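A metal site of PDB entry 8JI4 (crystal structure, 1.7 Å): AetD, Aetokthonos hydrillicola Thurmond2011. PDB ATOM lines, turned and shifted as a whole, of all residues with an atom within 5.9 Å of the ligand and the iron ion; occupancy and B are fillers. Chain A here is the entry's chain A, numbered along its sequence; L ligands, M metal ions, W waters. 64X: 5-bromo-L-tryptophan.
A ring nitrogen (ND1) of His 182 sits at hydrogen-bond distance from the backbone carbonyl oxygen (O) of Tyr 177, at 2.7 Å. OE1 of Glu 150 sits close to OE2 of Glu 186, 2.5 Å away.
Within 4 Å of the iron ion: His 89, His 182 and Glu 186. Along chain A the residues within 4 Å of the iron ion span positions 89 to 186.
Water W1 lies within hydrogen-bond range of an oxygen (OXT) of the ligand (2.8 Å), the backbone carbonyl oxygen (O) of Ala 55 (2.9 Å) and the backbone NH (N) of Trp 90 (3.4 Å).
The side-chain hydroxyl of Tyr 177 is in hydrogen-bond range of an oxygen (OXT) of the ligand (2.7 Å). A nitrogen (NE1) of the ligand is in hydrogen-bond range of the backbone carbonyl oxygen (O) of Met 149 (2.9 Å). The side-chain sulfur (SD) of Met 149 sits close to a nitrogen (NE1) of the ligand.
Residues that only touch the ligand: Phe 54, Phe 58, Glu 150, Gly 153, Ile 156 and Phe 157. 11 residues have an atom within 4 Å of the ligand: Phe 54, Phe 58, His 89, Met 149, Glu 150, Gly 153, Ile 156, Phe 157, Tyr 177, His 182 and Glu 186.
The iron ion is bound by an oxygen (O) of the ligand (2.1 Å), a ring nitrogen (ND1) of His 89 (2.1 Å), a ring nitrogen (NE2) of His 182 (2.1 Å), the side-chain carboxylate (OE1) of Glu 186 (2.1 Å), water W2 (2.1 Å) and a nitrogen (N) of the ligand (2.1 Å). The iron ion has six donor atoms within binding distance.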
ATOM      1  N   ILE A  51      23.541 -20.782  14.892  1.00  0.00           N
ATOM      2  CA  ILE A  51      24.523 -21.306  15.861  1.00  0.00           C
ATOM      3  C   ILE A  51      24.387 -22.845  15.966  1.00  0.00           C
ATOM      4  O   ILE A  51      25.313 -23.467  16.514  1.00  0.00           O
ATOM      5  CB  ILE A  51      24.335 -20.598  17.220  1.00  0.00           C
ATOM      6  CG1 ILE A  51      24.542 -19.089  17.018  1.00  0.00           C
ATOM      7  CG2 ILE A  51      25.299 -21.184  18.217  1.00  0.00           C
ATOM      8  CD1 ILE A  51      24.265 -18.269  18.254  1.00  0.00           C
ATOM      9  N   PHE A  54      27.260 -24.782  14.877  1.00  0.00           N
ATOM     10  CA  PHE A  54      28.482 -24.551  15.663  1.00  0.00           C
ATOM     11  C   PHE A  54      28.409 -25.220  17.074  1.00  0.00           C
ATOM     12  O   PHE A  54      29.421 -25.850  17.493  1.00  0.00           O
ATOM     13  CB  PHE A  54      28.731 -23.040  15.855  1.00  0.00           C
ATOM     14  CG  PHE A  54      29.821 -22.762  16.842  1.00  0.00           C
ATOM     15  CD1 PHE A  54      31.134 -22.723  16.465  1.00  0.00           C
ATOM     16  CD2 PHE A  54      29.483 -22.617  18.178  1.00  0.00           C
ATOM     17  CE1 PHE A  54      32.129 -22.564  17.405  1.00  0.00           C
ATOM     18  CE2 PHE A  54      30.470 -22.445  19.111  1.00  0.00           C
ATOM     19  CZ  PHE A  54      31.795 -22.394  18.729  1.00  0.00           C
ATOM     20  N   ALA A  55      27.325 -25.005  17.784  1.00  0.00           N
ATOM     21  CA  ALA A  55      27.340 -25.168  19.265  1.00  0.00           C
ATOM     22  C   ALA A  55      27.666 -26.623  19.686  1.00  0.00           C
ATOM     23  O   ALA A  55      28.407 -26.826  20.671  1.00  0.00           O
ATOM     24  CB  ALA A  55      26.082 -24.691  19.915  1.00  0.00           C
ATOM     25  N   PHE A  58      31.188 -27.455  18.992  1.00  0.00           N
ATOM     26  CA  PHE A  58      32.095 -26.880  19.996  1.00  0.00           C
ATOM     27  C   PHE A  58      32.137 -27.801  21.214  1.00  0.00           C
ATOM     28  O   PHE A  58      33.215 -28.030  21.756  1.00  0.00           O
ATOM     29  CB  PHE A  58      31.644 -25.467  20.390  1.00  0.00           C
ATOM     30  CG  PHE A  58      32.565 -24.790  21.347  1.00  0.00           C
ATOM     31  CD1 PHE A  58      33.841 -24.403  20.983  1.00  0.00           C
ATOM     32  CD2 PHE A  58      32.178 -24.647  22.663  1.00  0.00           C
ATOM     33  CE1 PHE A  58      34.674 -23.759  21.893  1.00  0.00           C
ATOM     34  CE2 PHE A  58      33.027 -24.031  23.587  1.00  0.00           C
ATOM     35  CZ  PHE A  58      34.264 -23.591  23.172  1.00  0.00           C
ATOM     36  N   ASP A  86      33.211 -25.743  29.765  1.00  0.00           N
ATOM     37  CA  ASP A  86      32.863 -25.116  28.468  1.00  0.00           C
ATOM     38  C   ASP A  86      32.016 -26.106  27.633  1.00  0.00           C
ATOM     39  O   ASP A  86      31.188 -25.610  26.871  1.00  0.00           O
ATOM     40  CB  ASP A  86      34.128 -24.627  27.774  1.00  0.00           C
ATOM     41  CG  ASP A  86      34.892 -23.573  28.587  1.00  0.00           C
ATOM     42  OD1 ASP A  86      34.285 -22.979  29.507  1.00  0.00           O
ATOM     43  OD2 ASP A  86      36.081 -23.398  28.315  1.00  0.00           O
ATOM     44  N   HIS A  89      27.785 -25.996  27.590  1.00  0.00           N
ATOM     45  CA  HIS A  89      26.995 -24.826  27.167  1.00  0.00           C
ATOM     46  C   HIS A  89      26.041 -25.177  26.022  1.00  0.00           C
ATOM     47  O   HIS A  89      25.006 -24.468  25.824  1.00  0.00           O
ATOM     48  CB  HIS A  89      27.934 -23.670  26.796  1.00  0.00           C
ATOM     49  CG  HIS A  89      28.745 -23.173  27.961  1.00  0.00           C
ATOM     50  ND1 HIS A  89      29.616 -22.125  27.831  1.00  0.00           N
ATOM     51  CD2 HIS A  89      28.837 -23.605  29.237  1.00  0.00           C
ATOM     52  CE1 HIS A  89      30.203 -21.912  28.998  1.00  0.00           C
ATOM     53  NE2 HIS A  89      29.767 -22.806  29.863  1.00  0.00           N
ATOM     54  N   TRP A  90      26.259 -26.297  25.313  1.00  0.00           N
ATOM     55  CA  TRP A  90      25.351 -26.643  24.210  1.00  0.00           C
ATOM     56  C   TRP A  90      23.929 -26.863  24.709  1.00  0.00           C
ATOM     57  O   TRP A  90      22.994 -26.628  23.997  1.00  0.00           O
ATOM     58  CB  TRP A  90      25.919 -27.859  23.476  1.00  0.00           C
ATOM     59  CG  TRP A  90      25.936 -29.088  24.319  1.00  0.00           C
ATOM     60  CD1 TRP A  90      26.809 -29.386  25.322  1.00  0.00           C
ATOM     61  CD2 TRP A  90      24.980 -30.163  24.298  1.00  0.00           C
ATOM     62  NE1 TRP A  90      26.497 -30.593  25.898  1.00  0.00           N
ATOM     63  CE2 TRP A  90      25.375 -31.084  25.290  1.00  0.00           C
ATOM     64  CE3 TRP A  90      23.845 -30.432  23.522  1.00  0.00           C
ATOM     65  CZ2 TRP A  90      24.697 -32.297  25.475  1.00  0.00           C
ATOM     66  CZ3 TRP A  90      23.154 -31.597  23.754  1.00  0.00           C
ATOM     67  CH2 TRP A  90      23.583 -32.492  24.729  1.00  0.00           C
ATOM     68  N   TRP A  92      22.458 -25.124  27.068  1.00  0.00           N
ATOM     69  CA  TRP A  92      21.931 -23.740  27.171  1.00  0.00           C
ATOM     70  C   TRP A  92      21.494 -23.246  25.780  1.00  0.00           C
ATOM     71  O   TRP A  92      20.397 -22.713  25.658  1.00  0.00           O
ATOM     72  CB  TRP A  92      22.955 -22.798  27.778  1.00  0.00           C
ATOM     73  CG  TRP A  92      23.486 -23.208  29.107  1.00  0.00           C
ATOM     74  CD1 TRP A  92      22.936 -24.105  29.987  1.00  0.00           C
ATOM     75  CD2 TRP A  92      24.629 -22.647  29.755  1.00  0.00           C
ATOM     76  NE1 TRP A  92      23.718 -24.192  31.117  1.00  0.00           N
ATOM     77  CE2 TRP A  92      24.718 -23.249  31.032  1.00  0.00           C
ATOM     78  CE3 TRP A  92      25.573 -21.669  29.406  1.00  0.00           C
ATOM     79  CZ2 TRP A  92      25.752 -22.952  31.911  1.00  0.00           C
ATOM     80  CZ3 TRP A  92      26.577 -21.350  30.288  1.00  0.00           C
ATOM     81  CH2 TRP A  92      26.657 -21.986  31.541  1.00  0.00           C
ATOM     82  N   LEU A 126      34.315 -24.090  11.791  1.00  0.00           N
ATOM     83  CA  LEU A 126      35.243 -23.387  12.705  1.00  0.00           C
ATOM     84  C   LEU A 126      35.856 -24.417  13.659  1.00  0.00           C
ATOM     85  O   LEU A 126      37.098 -24.445  13.816  1.00  0.00           O
ATOM     86  CB  LEU A 126      34.478 -22.308  13.478  1.00  0.00           C
ATOM     87  CG  LEU A 126      35.224 -21.628  14.614  1.00  0.00           C
ATOM     88  CD1 LEU A 126      36.563 -21.049  14.190  1.00  0.00           C
ATOM     89  CD2 LEU A 126      34.348 -20.509  15.170  1.00  0.00           C
ATOM     90  N   MET A 149      40.203 -18.385  20.997  1.00  0.00           N
ATOM     91  CA  MET A 149      38.843 -18.861  20.681  1.00  0.00           C
ATOM     92  C   MET A 149      37.867 -18.271  21.727  1.00  0.00           C
ATOM     93  O   MET A 149      36.763 -17.793  21.379  1.00  0.00           O
ATOM     94  CB  MET A 149      38.808 -20.379  20.637  1.00  0.00           C
ATOM     95  CG  MET A 149      37.439 -20.971  20.406  1.00  0.00           C
ATOM     96  SD  MET A 149      36.772 -20.359  18.829  1.00  0.00           S
ATOM     97  CE  MET A 149      35.355 -21.434  18.695  1.00  0.00           C
ATOM     98  N   GLU A 150      38.285 -18.296  22.975  1.00  0.00           N
ATOM     99  CA  GLU A 150      37.432 -17.813  24.097  1.00  0.00           C
ATOM    100  C   GLU A 150      37.270 -16.290  24.027  1.00  0.00           C
ATOM    101  O   GLU A 150      36.175 -15.809  24.338  1.00  0.00           O
ATOM    102  CB  GLU A 150      38.020 -18.296  25.419  1.00  0.00           C
ATOM    103  CG  GLU A 150      37.837 -19.796  25.596  1.00  0.00           C
ATOM    104  CD  GLU A 150      36.378 -20.232  25.613  1.00  0.00           C
ATOM    105  OE1 GLU A 150      35.679 -19.881  26.560  1.00  0.00           O
ATOM    106  OE2 GLU A 150      35.904 -20.821  24.616  1.00  0.00           O
ATOM    107  N   ALA A 152      37.238 -14.527  21.193  1.00  0.00           N
ATOM    108  CA  ALA A 152      36.222 -14.325  20.145  1.00  0.00           C
ATOM    109  C   ALA A 152      34.825 -14.644  20.708  1.00  0.00           C
ATOM    110  O   ALA A 152      33.920 -13.901  20.466  1.00  0.00           O
ATOM    111  CB  ALA A 152      36.543 -15.119  18.892  1.00  0.00           C
ATOM    112  N   GLY A 153      34.654 -15.739  21.433  1.00  0.00           N
ATOM    113  CA  GLY A 153      33.356 -16.159  22.029  1.00  0.00           C
ATOM    114  C   GLY A 153      32.782 -15.102  22.963  1.00  0.00           C
ATOM    115  O   GLY A 153      31.577 -14.814  22.907  1.00  0.00           O
ATOM    116  N   LEU A 154      33.630 -14.542  23.780  1.00  0.00           N
ATOM    117  CA  LEU A 154      33.208 -13.510  24.770  1.00  0.00           C
ATOM    118  C   LEU A 154      32.752 -12.255  24.063  1.00  0.00           C
ATOM    119  O   LEU A 154      31.787 -11.625  24.480  1.00  0.00           O
ATOM    120  CB  LEU A 154      34.346 -13.265  25.754  1.00  0.00           C
ATOM    121  CG  LEU A 154      34.553 -14.395  26.748  1.00  0.00           C
ATOM    122  CD1 LEU A 154      35.866 -14.230  27.503  1.00  0.00           C
ATOM    123  CD2 LEU A 154      33.366 -14.473  27.712  1.00  0.00           C
ATOM    124  N   ILE A 156      31.252 -12.298  21.088  1.00  0.00           N
ATOM    125  CA  ILE A 156      29.954 -12.630  20.522  1.00  0.00           C
ATOM    126  C   ILE A 156      28.864 -12.607  21.580  1.00  0.00           C
ATOM    127  O   ILE A 156      27.802 -12.081  21.332  1.00  0.00           O
ATOM    128  CB  ILE A 156      30.075 -13.980  19.811  1.00  0.00           C
ATOM    129  CG1 ILE A 156      31.023 -13.833  18.621  1.00  0.00           C
ATOM    130  CG2 ILE A 156      28.679 -14.480  19.448  1.00  0.00           C
ATOM    131  CD1 ILE A 156      31.478 -15.178  18.070  1.00  0.00           C
ATOM    132  N   PHE A 157      29.122 -13.266  22.680  1.00  0.00           N
ATOM    133  CA  PHE A 157      28.107 -13.467  23.732  1.00  0.00           C
ATOM    134  C   PHE A 157      27.904 -12.210  24.559  1.00  0.00           C
ATOM    135  O   PHE A 157      26.749 -11.995  24.957  1.00  0.00           O
ATOM    136  CB  PHE A 157      28.413 -14.748  24.493  1.00  0.00           C
ATOM    137  CG  PHE A 157      28.006 -15.931  23.655  1.00  0.00           C
ATOM    138  CD1 PHE A 157      26.695 -16.313  23.575  1.00  0.00           C
ATOM    139  CD2 PHE A 157      28.947 -16.562  22.869  1.00  0.00           C
ATOM    140  CE1 PHE A 157      26.342 -17.393  22.772  1.00  0.00           C
ATOM    141  CE2 PHE A 157      28.584 -17.592  22.018  1.00  0.00           C
ATOM    142  CZ  PHE A 157      27.275 -18.001  21.981  1.00  0.00           C
ATOM    143  N   TYR A 177      21.866 -18.996  27.411  1.00  0.00           N
ATOM    144  CA  TYR A 177      22.924 -18.986  26.381  1.00  0.00           C
ATOM    145  C   TYR A 177      23.170 -17.550  25.911  1.00  0.00           C
ATOM    146  O   TYR A 177      24.297 -17.109  25.963  1.00  0.00           O
ATOM    147  CB  TYR A 177      22.507 -19.900  25.220  1.00  0.00           C
ATOM    148  CG  TYR A 177      23.622 -20.248  24.262  1.00  0.00           C
ATOM    149  CD1 TYR A 177      24.721 -21.007  24.647  1.00  0.00           C
ATOM    150  CD2 TYR A 177      23.543 -19.854  22.942  1.00  0.00           C
ATOM    151  CE1 TYR A 177      25.714 -21.378  23.758  1.00  0.00           C
ATOM    152  CE2 TYR A 177      24.521 -20.204  22.027  1.00  0.00           C
ATOM    153  CZ  TYR A 177      25.607 -20.950  22.436  1.00  0.00           C
ATOM    154  OH  TYR A 177      26.562 -21.324  21.530  1.00  0.00           O
ATOM    155  N   HIS A 182      26.007 -16.644  30.985  1.00  0.00           N
ATOM    156  CA  HIS A 182      26.947 -17.360  30.081  1.00  0.00           C
ATOM    157  C   HIS A 182      28.285 -16.594  30.016  1.00  0.00           C
ATOM    158  O   HIS A 182      29.352 -17.212  30.167  1.00  0.00           O
ATOM    159  CB  HIS A 182      26.265 -17.532  28.721  1.00  0.00           C
ATOM    160  CG  HIS A 182      27.040 -18.324  27.721  1.00  0.00           C
ATOM    161  ND1 HIS A 182      26.587 -18.466  26.407  1.00  0.00           N
ATOM    162  CD2 HIS A 182      28.212 -19.014  27.798  1.00  0.00           C
ATOM    163  CE1 HIS A 182      27.443 -19.225  25.743  1.00  0.00           C
ATOM    164  NE2 HIS A 182      28.470 -19.559  26.541  1.00  0.00           N
ATOM    165  N   GLU A 186      31.738 -18.104  31.569  1.00  0.00           N
ATOM    166  CA  GLU A 186      32.778 -18.359  30.537  1.00  0.00           C
ATOM    167  C   GLU A 186      34.080 -17.683  30.949  1.00  0.00           C
ATOM    168  O   GLU A 186      35.144 -18.331  30.863  1.00  0.00           O
ATOM    169  CB  GLU A 186      32.350 -17.888  29.149  1.00  0.00           C
ATOM    170  CG  GLU A 186      33.219 -18.510  28.054  1.00  0.00           C
ATOM    171  CD  GLU A 186      32.541 -19.645  27.310  1.00  0.00           C
ATOM    172  OE1 GLU A 186      31.320 -19.717  27.421  1.00  0.00           O
ATOM    173  OE2 GLU A 186      33.246 -20.391  26.564  1.00  0.00           O
ATOM    174  N   SER A 224      36.815 -17.060  12.901  1.00  0.00           N
ATOM    175  CA  SER A 224      35.697 -16.500  13.689  1.00  0.00           C
ATOM    176  C   SER A 224      35.011 -15.375  12.888  1.00  0.00           C
ATOM    177  O   SER A 224      33.788 -15.261  12.873  1.00  0.00           O
ATOM    178  CB  SER A 224      36.208 -16.034  15.044  1.00  0.00           C
ATOM    179  OG  SER A 224      36.639 -17.137  15.803  1.00  0.00           O
ATOM    180  N   LEU A 227      32.806 -16.971  10.185  1.00  0.00           N
ATOM    181  CA  LEU A 227      31.534 -17.341  10.846  1.00  0.00           C
ATOM    182  C   LEU A 227      30.631 -16.099  10.958  1.00  0.00           C
ATOM    183  O   LEU A 227      29.468 -16.171  10.519  1.00  0.00           O
ATOM    184  CB  LEU A 227      31.830 -18.030  12.198  1.00  0.00           C
ATOM    185  CG  LEU A 227      30.624 -18.383  13.069  1.00  0.00           C
ATOM    186  CD1 LEU A 227      31.026 -19.466  14.068  1.00  0.00           C
ATOM    187  CD2 LEU A 227      30.085 -17.154  13.824  1.00  0.00           C
ATOM    188  N   PHE A 231      26.712 -15.062   9.538  1.00  0.00           N
ATOM    189  CA  PHE A 231      25.597 -14.612  10.393  1.00  0.00           C
ATOM    190  C   PHE A 231      25.031 -13.324   9.778  1.00  0.00           C
ATOM    191  O   PHE A 231      23.819 -13.202   9.682  1.00  0.00           O
ATOM    192  CB  PHE A 231      26.024 -14.438  11.855  1.00  0.00           C
ATOM    193  CG  PHE A 231      26.254 -15.685  12.671  1.00  0.00           C
ATOM    194  CD1 PHE A 231      26.410 -16.918  12.072  1.00  0.00           C
ATOM    195  CD2 PHE A 231      26.290 -15.618  14.046  1.00  0.00           C
ATOM    196  CE1 PHE A 231      26.625 -18.051  12.842  1.00  0.00           C
ATOM    197  CE2 PHE A 231      26.564 -16.736  14.829  1.00  0.00           C
ATOM    198  CZ  PHE A 231      26.682 -17.963  14.216  1.00  0.00           C
HETATM  199  OXT 64X L   1      28.845 -22.333  22.562  1.00  0.00           O
HETATM  200  C   64X L   1      29.372 -21.712  23.557  1.00  0.00           C
HETATM  201  O   64X L   1      28.996 -21.952  24.724  1.00  0.00           O
HETATM  202  CA  64X L   1      30.337 -20.534  23.241  1.00  0.00           C
HETATM  203  N   64X L   1      30.673 -19.791  24.467  1.00  0.00           N
HETATM  204  CB  64X L   1      31.583 -21.066  22.655  1.00  0.00           C
HETATM  205  CG  64X L   1      32.451 -20.131  21.763  1.00  0.00           C
HETATM  206  CD2 64X L   1      32.097 -19.560  20.563  1.00  0.00           C
HETATM  207  CE3 64X L   1      30.945 -19.458  19.737  1.00  0.00           C
HETATM  208  CZ3 64X L   1      30.904 -18.810  18.419  1.00  0.00           C
HETATM  209 BR1  64X L   1      29.268 -18.694  17.589  1.00  0.00          BR
HETATM  210  CH2 64X L   1      32.166 -18.268  18.099  1.00  0.00           C
HETATM  211  CZ2 64X L   1      33.314 -18.384  18.876  1.00  0.00           C
HETATM  212  CE2 64X L   1      33.245 -18.999  20.114  1.00  0.00           C
HETATM  213  NE1 64X L   1      34.228 -19.195  20.945  1.00  0.00           N
HETATM  214  CD1 64X L   1      33.760 -19.916  22.008  1.00  0.00           C
HETATM  215 FE    FE M   1      30.053 -20.899  26.184  1.00  0.00          FE
HETATM  216  O   HOH W   1      28.267 -25.033  22.929  1.00  0.00           O
HETATM  217  O   HOH W   2      31.652 -22.270  25.850  1.00  0.00           O
